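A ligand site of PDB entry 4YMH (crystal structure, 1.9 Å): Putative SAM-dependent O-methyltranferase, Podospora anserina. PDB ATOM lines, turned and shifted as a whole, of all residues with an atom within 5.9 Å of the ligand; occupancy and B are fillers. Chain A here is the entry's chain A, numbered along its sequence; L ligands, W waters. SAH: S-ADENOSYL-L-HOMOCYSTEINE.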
ATOM      1  N   LYS A  47     -14.546   5.255  11.894  1.00  0.00           N
ATOM      2  CA  LYS A  47     -15.802   4.868  11.260  1.00  0.00           C
ATOM      3  C   LYS A  47     -15.733   3.481  10.637  1.00  0.00           C
ATOM      4  O   LYS A  47     -16.758   2.827  10.429  1.00  0.00           O
ATOM      5  CB  LYS A  47     -16.201   5.871  10.168  1.00  0.00           C
ATOM      6  CG  LYS A  47     -16.472   7.282  10.643  1.00  0.00           C
ATOM      7  CD  LYS A  47     -17.003   8.124   9.502  1.00  0.00           C
ATOM      8  CE  LYS A  47     -17.276   9.554   9.931  1.00  0.00           C
ATOM      9  NZ  LYS A  47     -17.964  10.312   8.862  1.00  0.00           N
ATOM     10  N   MET A  48     -14.517   3.031  10.322  1.00  0.00           N
ATOM     11  CA  MET A  48     -14.327   1.735   9.684  1.00  0.00           C
ATOM     12  C   MET A  48     -14.480   0.583  10.678  1.00  0.00           C
ATOM     13  O   MET A  48     -14.142   0.722  11.852  1.00  0.00           O
ATOM     14  CB  MET A  48     -12.950   1.671   9.004  1.00  0.00           C
ATOM     15  CG  MET A  48     -12.638   0.365   8.305  1.00  0.00           C
ATOM     16  SD  MET A  48     -11.132   0.544   7.342  1.00  0.00           S
ATOM     17  CE  MET A  48     -10.016   1.152   8.606  1.00  0.00           C
ATOM     18  N   SER A  49     -15.008  -0.546  10.203  1.00  0.00           N
ATOM     19  CA  SER A  49     -15.146  -1.733  11.047  1.00  0.00           C
ATOM     20  C   SER A  49     -13.764  -2.240  11.456  1.00  0.00           C
ATOM     21  O   SER A  49     -12.767  -1.870  10.845  1.00  0.00           O
ATOM     22  CB  SER A  49     -15.941  -2.816  10.309  1.00  0.00           C
ATOM     23  OG  SER A  49     -17.235  -2.325   9.983  1.00  0.00           O
ATOM     24  N   MET A  57     -17.976 -10.685   8.869  1.00  0.00           N
ATOM     25  CA  MET A  57     -18.696 -10.435   7.637  1.00  0.00           C
ATOM     26  C   MET A  57     -18.402 -11.525   6.616  1.00  0.00           C
ATOM     27  O   MET A  57     -19.322 -12.050   5.977  1.00  0.00           O
ATOM     28  CB  MET A  57     -18.321  -9.052   7.066  1.00  0.00           C
ATOM     29  CG  MET A  57     -18.775  -7.900   7.961  1.00  0.00           C
ATOM     30  SD  MET A  57     -18.278  -6.299   7.301  1.00  0.00           S
ATOM     31  CE  MET A  57     -16.555  -6.299   7.609  1.00  0.00           C
ATOM     32  N   GLU A  71     -25.494  -2.813   0.872  1.00  0.00           N
ATOM     33  CA  GLU A  71     -24.813  -2.154   1.965  1.00  0.00           C
ATOM     34  C   GLU A  71     -25.113  -0.661   1.944  1.00  0.00           C
ATOM     35  O   GLU A  71     -25.050  -0.016   0.904  1.00  0.00           O
ATOM     36  CB  GLU A  71     -23.311  -2.431   1.856  1.00  0.00           C
ATOM     37  CG  GLU A  71     -22.427  -1.393   2.479  1.00  0.00           C
ATOM     38  CD  GLU A  71     -20.976  -1.806   2.429  1.00  0.00           C
ATOM     39  OE1 GLU A  71     -20.172  -1.117   1.745  1.00  0.00           O
ATOM     40  OE2 GLU A  71     -20.636  -2.809   3.084  1.00  0.00           O
ATOM     41  N   ILE A  72     -25.466  -0.102   3.088  1.00  0.00           N
ATOM     42  CA  ILE A  72     -25.747   1.329   3.170  1.00  0.00           C
ATOM     43  C   ILE A  72     -24.625   1.948   4.010  1.00  0.00           C
ATOM     44  O   ILE A  72     -24.514   1.652   5.204  1.00  0.00           O
ATOM     45  CB  ILE A  72     -27.130   1.616   3.777  1.00  0.00           C
ATOM     46  CG1 ILE A  72     -28.199   0.773   3.070  1.00  0.00           C
ATOM     47  CG2 ILE A  72     -27.466   3.093   3.657  1.00  0.00           C
ATOM     48  CD1 ILE A  72     -29.628   1.011   3.581  1.00  0.00           C
ATOM     49  N   GLY A  73     -23.797   2.774   3.367  1.00  0.00           N
ATOM     50  CA  GLY A  73     -22.658   3.398   4.012  1.00  0.00           C
ATOM     51  C   GLY A  73     -21.367   2.687   3.631  1.00  0.00           C
ATOM     52  O   GLY A  73     -20.969   1.710   4.260  1.00  0.00           O
ATOM     53  N   CYS A  74     -20.706   3.171   2.580  1.00  0.00           N
ATOM     54  CA  CYS A  74     -19.533   2.486   2.035  1.00  0.00           C
ATOM     55  C   CYS A  74     -18.233   2.893   2.736  1.00  0.00           C
ATOM     56  O   CYS A  74     -17.349   2.053   2.924  1.00  0.00           O
ATOM     57  CB  CYS A  74     -19.427   2.762   0.529  1.00  0.00           C
ATOM     58  SG  CYS A  74     -18.132   1.825  -0.305  1.00  0.00           S
ATOM     59  N   TYR A  75     -18.154   4.159   3.147  1.00  0.00           N
ATOM     60  CA  TYR A  75     -16.913   4.790   3.632  1.00  0.00           C
ATOM     61  C   TYR A  75     -15.758   4.523   2.672  1.00  0.00           C
ATOM     62  O   TYR A  75     -15.776   5.006   1.540  1.00  0.00           O
ATOM     63  CB  TYR A  75     -16.561   4.317   5.035  1.00  0.00           C
ATOM     64  CG  TYR A  75     -15.491   5.146   5.698  1.00  0.00           C
ATOM     65  CD1 TYR A  75     -15.651   6.521   5.855  1.00  0.00           C
ATOM     66  CD2 TYR A  75     -14.308   4.572   6.156  1.00  0.00           C
ATOM     67  CE1 TYR A  75     -14.671   7.303   6.457  1.00  0.00           C
ATOM     68  CE2 TYR A  75     -13.320   5.353   6.764  1.00  0.00           C
ATOM     69  CZ  TYR A  75     -13.515   6.707   6.913  1.00  0.00           C
ATOM     70  OH  TYR A  75     -12.543   7.482   7.506  1.00  0.00           O
ATOM     71  N   SER A  76     -14.758   3.747   3.092  1.00  0.00           N
ATOM     72  CA  SER A  76     -13.597   3.497   2.223  1.00  0.00           C
ATOM     73  C   SER A  76     -13.664   2.173   1.453  1.00  0.00           C
ATOM     74  O   SER A  76     -12.749   1.821   0.716  1.00  0.00           O
ATOM     75  CB  SER A  76     -12.296   3.539   3.022  1.00  0.00           C
ATOM     76  OG  SER A  76     -12.035   2.293   3.653  1.00  0.00           O
ATOM     77  N   GLY A  77     -14.767   1.440   1.612  1.00  0.00           N
ATOM     78  CA  GLY A  77     -14.973   0.193   0.896  1.00  0.00           C
ATOM     79  C   GLY A  77     -14.595  -1.081   1.638  1.00  0.00           C
ATOM     80  O   GLY A  77     -14.685  -2.172   1.089  1.00  0.00           O
ATOM     81  N   TYR A  78     -14.149  -0.944   2.888  1.00  0.00           N
ATOM     82  CA  TYR A  78     -13.720  -2.114   3.675  1.00  0.00           C
ATOM     83  C   TYR A  78     -14.781  -3.193   3.812  1.00  0.00           C
ATOM     84  O   TYR A  78     -14.498  -4.378   3.555  1.00  0.00           O
ATOM     85  CB  TYR A  78     -13.277  -1.662   5.081  1.00  0.00           C
ATOM     86  CG  TYR A  78     -12.928  -2.793   6.025  1.00  0.00           C
ATOM     87  CD1 TYR A  78     -11.788  -3.579   5.804  1.00  0.00           C
ATOM     88  CD2 TYR A  78     -13.708  -3.071   7.137  1.00  0.00           C
ATOM     89  CE1 TYR A  78     -11.458  -4.606   6.677  1.00  0.00           C
ATOM     90  CE2 TYR A  78     -13.383  -4.111   8.013  1.00  0.00           C
ATOM     91  CZ  TYR A  78     -12.250  -4.868   7.774  1.00  0.00           C
ATOM     92  OH  TYR A  78     -11.908  -5.897   8.628  1.00  0.00           O
ATOM     93  N   SER A  79     -15.997  -2.815   4.200  1.00  0.00           N
ATOM     94  CA  SER A  79     -17.028  -3.835   4.385  1.00  0.00           C
ATOM     95  C   SER A  79     -17.518  -4.364   3.029  1.00  0.00           C
ATOM     96  O   SER A  79     -17.798  -5.554   2.902  1.00  0.00           O
ATOM     97  CB  SER A  79     -18.212  -3.330   5.234  1.00  0.00           C
ATOM     98  OG  SER A  79     -18.791  -2.145   4.728  1.00  0.00           O
ATOM     99  N   LEU A  97     -24.128   1.840  -1.054  1.00  0.00           N
ATOM    100  CA  LEU A  97     -24.610   3.213  -1.183  1.00  0.00           C
ATOM    101  C   LEU A  97     -23.745   4.191  -0.416  1.00  0.00           C
ATOM    102  O   LEU A  97     -23.419   3.931   0.751  1.00  0.00           O
ATOM    103  CB  LEU A  97     -26.061   3.318  -0.695  1.00  0.00           C
ATOM    104  CG  LEU A  97     -27.084   2.371  -1.298  1.00  0.00           C
ATOM    105  CD1 LEU A  97     -28.460   2.693  -0.749  1.00  0.00           C
ATOM    106  CD2 LEU A  97     -27.067   2.467  -2.831  1.00  0.00           C
ATOM    107  N   GLU A  98     -23.394   5.329  -1.025  1.00  0.00           N
ATOM    108  CA  GLU A  98     -22.537   6.281  -0.328  1.00  0.00           C
ATOM    109  C   GLU A  98     -22.801   7.716  -0.784  1.00  0.00           C
ATOM    110  O   GLU A  98     -23.039   7.935  -1.971  1.00  0.00           O
ATOM    111  CB  GLU A  98     -21.056   5.916  -0.545  1.00  0.00           C
ATOM    112  CG  GLU A  98     -20.065   6.956  -0.015  1.00  0.00           C
ATOM    113  CD  GLU A  98     -20.143   7.131   1.507  1.00  0.00           C
ATOM    114  OE1 GLU A  98     -20.128   6.119   2.238  1.00  0.00           O
ATOM    115  OE2 GLU A  98     -20.210   8.302   1.967  1.00  0.00           O
ATOM    116  N   TYR A  99     -22.718   8.682   0.097  1.00  0.00           N
ATOM    117  CA  TYR A  99     -22.945  10.072  -0.298  1.00  0.00           C
ATOM    118  C   TYR A  99     -21.765  11.015  -0.267  1.00  0.00           C
ATOM    119  O   TYR A  99     -21.799  12.031  -0.853  1.00  0.00           O
ATOM    120  CB  TYR A  99     -24.130  10.682   0.453  1.00  0.00           C
ATOM    121  CG  TYR A  99     -23.825  11.292   1.766  1.00  0.00           C
ATOM    122  CD1 TYR A  99     -24.492  12.425   2.197  1.00  0.00           C
ATOM    123  CD2 TYR A  99     -22.917  10.732   2.624  1.00  0.00           C
ATOM    124  CE1 TYR A  99     -24.256  12.966   3.428  1.00  0.00           C
ATOM    125  CE2 TYR A  99     -22.653  11.277   3.851  1.00  0.00           C
ATOM    126  CZ  TYR A  99     -23.321  12.387   4.257  1.00  0.00           C
ATOM    127  OH  TYR A  99     -23.078  12.945   5.501  1.00  0.00           O
ATOM    128  N   SER A 100     -20.729  10.648   0.429  1.00  0.00           N
ATOM    129  CA  SER A 100     -19.583  11.565   0.543  1.00  0.00           C
ATOM    130  C   SER A 100     -18.649  11.495  -0.670  1.00  0.00           C
ATOM    131  O   SER A 100     -18.066  10.447  -0.925  1.00  0.00           O
ATOM    132  CB  SER A 100     -18.786  11.265   1.807  1.00  0.00           C
ATOM    133  OG  SER A 100     -17.495  11.862   1.747  1.00  0.00           O
ATOM    134  N   MET A 103     -15.275  10.019   0.048  1.00  0.00           N
ATOM    135  CA  MET A 103     -15.262   8.569   0.290  1.00  0.00           C
ATOM    136  C   MET A 103     -15.622   7.783  -0.972  1.00  0.00           C
ATOM    137  O   MET A 103     -15.150   6.680  -1.161  1.00  0.00           O
ATOM    138  CB  MET A 103     -16.217   8.188   1.438  1.00  0.00           C
ATOM    139  CG  MET A 103     -15.818   8.789   2.789  1.00  0.00           C
ATOM    140  SD  MET A 103     -14.034   9.014   3.032  1.00  0.00           S
ATOM    141  CE  MET A 103     -13.437   7.313   3.107  1.00  0.00           C
ATOM    142  N   GLY A 125     -24.950   9.170  -3.769  1.00  0.00           N
ATOM    143  CA  GLY A 125     -26.050  10.049  -3.451  1.00  0.00           C
ATOM    144  C   GLY A 125     -26.615   9.734  -2.083  1.00  0.00           C
ATOM    145  O   GLY A 125     -26.304   8.687  -1.509  1.00  0.00           O
ATOM    146  N   PRO A 126     -27.462  10.647  -1.567  1.00  0.00           N
ATOM    147  CA  PRO A 126     -28.118  10.422  -0.276  1.00  0.00           C
ATOM    148  C   PRO A 126     -28.864   9.109  -0.308  1.00  0.00           C
ATOM    149  O   PRO A 126     -29.733   8.956  -1.161  1.00  0.00           O
ATOM    150  CB  PRO A 126     -29.104  11.598  -0.161  1.00  0.00           C
ATOM    151  CG  PRO A 126     -28.655  12.601  -1.193  1.00  0.00           C
ATOM    152  CD  PRO A 126     -28.008  11.812  -2.283  1.00  0.00           C
ATOM    153  N   ALA A 127     -28.535   8.178   0.595  1.00  0.00           N
ATOM    154  CA  ALA A 127     -29.125   6.848   0.575  1.00  0.00           C
ATOM    155  C   ALA A 127     -30.642   6.883   0.747  1.00  0.00           C
ATOM    156  O   ALA A 127     -31.339   5.982   0.268  1.00  0.00           O
ATOM    157  CB  ALA A 127     -28.502   5.980   1.639  1.00  0.00           C
ATOM    158  N   GLU A 128     -31.147   7.899   1.437  1.00  0.00           N
ATOM    159  CA  GLU A 128     -32.575   8.007   1.681  1.00  0.00           C
ATOM    160  C   GLU A 128     -33.339   8.041   0.359  1.00  0.00           C
ATOM    161  O   GLU A 128     -34.412   7.443   0.246  1.00  0.00           O
ATOM    162  CB  GLU A 128     -32.890   9.223   2.547  1.00  0.00           C
ATOM    163  CG  GLU A 128     -32.309  10.553   2.088  1.00  0.00           C
ATOM    164  CD  GLU A 128     -30.965  10.942   2.734  1.00  0.00           C
ATOM    165  OE1 GLU A 128     -30.191  10.060   3.138  1.00  0.00           O
ATOM    166  OE2 GLU A 128     -30.712  12.164   2.855  1.00  0.00           O
ATOM    167  N   PHE A 142     -26.698  -4.786   4.926  1.00  0.00           N
ATOM    168  CA  PHE A 142     -25.854  -4.245   5.991  1.00  0.00           C
ATOM    169  C   PHE A 142     -26.101  -2.743   6.116  1.00  0.00           C
ATOM    170  O   PHE A 142     -25.741  -1.991   5.207  1.00  0.00           O
ATOM    171  CB  PHE A 142     -24.378  -4.536   5.672  1.00  0.00           C
ATOM    172  CG  PHE A 142     -23.408  -4.137   6.762  1.00  0.00           C
ATOM    173  CD1 PHE A 142     -23.591  -4.567   8.077  1.00  0.00           C
ATOM    174  CD2 PHE A 142     -22.272  -3.397   6.459  1.00  0.00           C
ATOM    175  CE1 PHE A 142     -22.673  -4.222   9.079  1.00  0.00           C
ATOM    176  CE2 PHE A 142     -21.350  -3.053   7.437  1.00  0.00           C
ATOM    177  CZ  PHE A 142     -21.556  -3.464   8.757  1.00  0.00           C
ATOM    178  N   ASP A 144     -25.134   0.651   7.795  1.00  0.00           N
ATOM    179  CA  ASP A 144     -23.998   1.194   8.532  1.00  0.00           C
ATOM    180  C   ASP A 144     -23.773   2.657   8.165  1.00  0.00           C
ATOM    181  O   ASP A 144     -22.640   3.098   8.118  1.00  0.00           O
ATOM    182  CB  ASP A 144     -22.759   0.342   8.248  1.00  0.00           C
ATOM    183  CG  ASP A 144     -21.599   0.613   9.206  1.00  0.00           C
ATOM    184  OD1 ASP A 144     -21.809   1.181  10.299  1.00  0.00           O
ATOM    185  OD2 ASP A 144     -20.441   0.274   8.847  1.00  0.00           O
ATOM    186  N   ALA A 145     -24.838   3.400   7.895  1.00  0.00           N
ATOM    187  CA  ALA A 145     -24.718   4.805   7.467  1.00  0.00           C
ATOM    188  C   ALA A 145     -25.051   5.793   8.597  1.00  0.00           C
ATOM    189  O   ALA A 145     -24.702   5.570   9.758  1.00  0.00           O
ATOM    190  CB  ALA A 145     -25.594   5.067   6.259  1.00  0.00           C
ATOM    191  N   ASN A 146     -25.742   6.892   8.259  1.00  0.00           N
ATOM    192  CA  ASN A 146     -26.107   7.877   9.286  1.00  0.00           C
ATOM    193  C   ASN A 146     -27.093   7.255  10.277  1.00  0.00           C
ATOM    194  O   ASN A 146     -28.125   6.688   9.880  1.00  0.00           O
ATOM    195  CB  ASN A 146     -26.697   9.146   8.652  1.00  0.00           C
ATOM    196  CG  ASN A 146     -27.782   8.838   7.639  1.00  0.00           C
ATOM    197  OD1 ASN A 146     -27.608   7.977   6.780  1.00  0.00           O
ATOM    198  ND2 ASN A 146     -28.920   9.528   7.752  1.00  0.00           N
ATOM    199  N   LYS A 147     -26.763   7.327  11.559  1.00  0.00           N
ATOM    200  CA  LYS A 147     -27.529   6.614  12.574  1.00  0.00           C
ATOM    201  C   LYS A 147     -28.955   7.154  12.661  1.00  0.00           C
ATOM    202  O   LYS A 147     -29.873   6.408  13.014  1.00  0.00           O
ATOM    203  CB  LYS A 147     -26.845   6.677  13.936  1.00  0.00           C
ATOM    204  CG  LYS A 147     -25.353   6.310  13.910  1.00  0.00           C
ATOM    205  CD  LYS A 147     -25.090   4.914  13.318  1.00  0.00           C
ATOM    206  CE  LYS A 147     -23.579   4.707  13.142  1.00  0.00           C
ATOM    207  NZ  LYS A 147     -23.273   3.856  11.963  1.00  0.00           N
ATOM    208  N   TYR A 153     -34.474   3.830   6.621  1.00  0.00           N
ATOM    209  CA  TYR A 153     -33.938   2.835   5.699  1.00  0.00           C
ATOM    210  C   TYR A 153     -34.721   1.525   5.839  1.00  0.00           C
ATOM    211  O   TYR A 153     -35.186   0.947   4.846  1.00  0.00           O
ATOM    212  CB  TYR A 153     -32.452   2.594   5.949  1.00  0.00           C
ATOM    213  CG  TYR A 153     -31.594   3.798   5.658  1.00  0.00           C
ATOM    214  CD1 TYR A 153     -31.867   4.631   4.580  1.00  0.00           C
ATOM    215  CD2 TYR A 153     -30.509   4.115   6.465  1.00  0.00           C
ATOM    216  CE1 TYR A 153     -31.081   5.740   4.298  1.00  0.00           C
ATOM    217  CE2 TYR A 153     -29.707   5.229   6.197  1.00  0.00           C
ATOM    218  CZ  TYR A 153     -30.007   6.040   5.116  1.00  0.00           C
ATOM    219  OH  TYR A 153     -29.229   7.151   4.829  1.00  0.00           O
ATOM    220  N   ASP A 172     -25.458  -1.993  12.150  1.00  0.00           N
ATOM    221  CA  ASP A 172     -24.212  -1.853  12.914  1.00  0.00           C
ATOM    222  C   ASP A 172     -24.205  -0.613  13.827  1.00  0.00           C
ATOM    223  O   ASP A 172     -24.917   0.367  13.563  1.00  0.00           O
ATOM    224  CB  ASP A 172     -23.038  -1.801  11.944  1.00  0.00           C
ATOM    225  CG  ASP A 172     -21.751  -2.249  12.560  1.00  0.00           C
ATOM    226  OD1 ASP A 172     -21.800  -3.061  13.509  1.00  0.00           O
ATOM    227  OD2 ASP A 172     -20.682  -1.788  12.109  1.00  0.00           O
HETATM  228  N   SAH L   1     -19.309   0.334   6.260  1.00  0.00           N
HETATM  229  CA  SAH L   1     -18.023   0.942   6.438  1.00  0.00           C
HETATM  230  CB  SAH L   1     -18.110   2.205   7.280  1.00  0.00           C
HETATM  231  CG  SAH L   1     -19.309   3.128   7.049  1.00  0.00           C
HETATM  232  SD  SAH L   1     -19.151   4.604   7.966  1.00  0.00           S
HETATM  233  C   SAH L   1     -17.060  -0.008   7.092  1.00  0.00           C
HETATM  234  O   SAH L   1     -15.866   0.170   6.982  1.00  0.00           O
HETATM  235  OXT SAH L   1     -17.496  -0.951   7.741  1.00  0.00           O
HETATM  236  C5' SAH L   1     -20.624   5.370   7.439  1.00  0.00           C
HETATM  237  C4' SAH L   1     -20.595   5.889   6.015  1.00  0.00           C
HETATM  238  O4' SAH L   1     -21.895   6.303   5.636  1.00  0.00           O
HETATM  239  C3' SAH L   1     -19.717   7.098   5.845  1.00  0.00           C
HETATM  240  O3' SAH L   1     -18.774   6.912   4.810  1.00  0.00           O
HETATM  241  C2' SAH L   1     -20.667   8.219   5.489  1.00  0.00           C
HETATM  242  O2' SAH L   1     -20.106   9.197   4.670  1.00  0.00           O
HETATM  243  C1' SAH L   1     -21.836   7.492   4.880  1.00  0.00           C
HETATM  244  N9  SAH L   1     -23.113   8.218   5.015  1.00  0.00           N
HETATM  245  C8  SAH L   1     -23.527   8.957   6.026  1.00  0.00           C
HETATM  246  N7  SAH L   1     -24.732   9.440   5.786  1.00  0.00           N
HETATM  247  C5  SAH L   1     -25.112   9.009   4.607  1.00  0.00           C
HETATM  248  C6  SAH L   1     -26.281   9.150   3.751  1.00  0.00           C
HETATM  249  N6  SAH L   1     -27.286   9.884   4.177  1.00  0.00           N
HETATM  250  N1  SAH L   1     -26.308   8.523   2.579  1.00  0.00           N
HETATM  251  C2  SAH L   1     -25.282   7.786   2.192  1.00  0.00           C
HETATM  252  N3  SAH L   1     -24.182   7.603   2.900  1.00  0.00           N
HETATM  253  C4  SAH L   1     -24.043   8.181   4.105  1.00  0.00           C
HETATM  254  O   HOH W   1     -14.486   1.414   4.930  1.00  0.00           O
HETATM  255  O   HOH W   2     -26.465  11.764   6.518  1.00  0.00           O
HETATM  256  O   HOH W   3     -17.751   9.766   6.046  1.00  0.00           O
HETATM  257  O   HOH W   4     -19.955   3.630  10.990  1.00  0.00           O
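The backbone NH of Ser 49 is in hydrogen-bond range of an oxygen (O) of the ligand (3.4 Å).
OG of Ser 49 lies within hydrogen-bond range of OXT of the ligand (2.6 Å).
The side-chain carboxylate (OD2) of Asp 144 is in salt-bridge range of a nitrogen (N) of the ligand (2.8 Å).
O2' of the ligand lies within hydrogen-bond range of OE2 of Glu 98 (2.8 Å).
O of Gly 73 lies within hydrogen-bond range of N of the ligand (2.9 Å).
A nitrogen (N) of the ligand lies within hydrogen-bond range of the side-chain hydroxyl (OG) of Ser 79, 3.0 Å away.
The backbone NH (N) of Ala 127 is in hydrogen-bond range of a nitrogen (N1) of the ligand (3.0 Å).
N of Tyr 75 lies close to O3' of the ligand.
The side-chain carboxylate (OE1) of Glu 128 sits at hydrogen-bond distance from a nitrogen (N6) of the ligand.
A nitrogen (N3) of the ligand sits at hydrogen-bond distance from the backbone NH (N) of Tyr 99.
A nitrogen (N6) of the ligand sits at hydrogen-bond distance from the side-chain amide oxygen (OD1) of Asn 146 (3.2 Å).
OH of Tyr 153 is in hydrogen-bond range of N6 of the ligand.
The side-chain carboxylate (OE1) of Glu 98 lies within hydrogen-bond range of the backbone NH (N) of Cys 74, 3.0 Å away.
The side-chain carboxylate (OE2) of Glu 98 sits at hydrogen-bond distance from the backbone NH (N) of Ser 100 (2.9 Å).
The backbone carbonyl oxygen of Glu 98 is in hydrogen-bond range of the backbone NH of Gly 125 (2.9 Å).
O of Leu 97 is in hydrogen-bond range of N of Gly 73 (2.9 Å).
The side-chain carboxylate (OE2) of Glu 71 is in hydrogen-bond range of the side-chain hydroxyl (OG) of Ser 79, 2.6 Å away.
O of Ala 145 is in hydrogen-bond range of NZ of Lys 147 (3.1 Å).
O of Leu 97 sits at hydrogen-bond distance from N of Cys 74, at 3.4 Å.
OG of Ser 100 lies within hydrogen-bond range of N of Met 103, at 3.3 Å.
Merely in contact with the ligand: Met 48, Lys 47, Ala 145, Tyr 78, Cys 74, Ser 100, Pro 126 and Gly 125.
Hydrophobic or aromatic side chains that line the ligand: Met 48, Tyr 75, Tyr 78, Tyr 99, Ala 127 and Ala 145.
19 residues have an atom within 4 Å of the ligand: Lys 47, Met 48, Ser 49, Gly 73, Cys 74, Tyr 75, Tyr 78, Ser 79, Glu 98, Tyr 99, Ser 100, Gly 125, Pro 126, Ala 127, Glu 128, Asp 144, Ala 145, Asn 146 and Tyr 153.
The nearest printed residue that does not touch the ligand is Met 103 (4.04 Å).
Water W1 lies within hydrogen-bond range of an oxygen (O) of the ligand (2.8 Å), the side-chain hydroxyl (OG) of Ser 76 (2.9 Å), the backbone NH (N) of Tyr 78 (3.1 Å) and the backbone NH (N) of Gly 77 (3.3 Å).
Water W3 lies within hydrogen-bond range of an oxygen (O2') of the ligand and the side-chain amino group of Lys 47.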
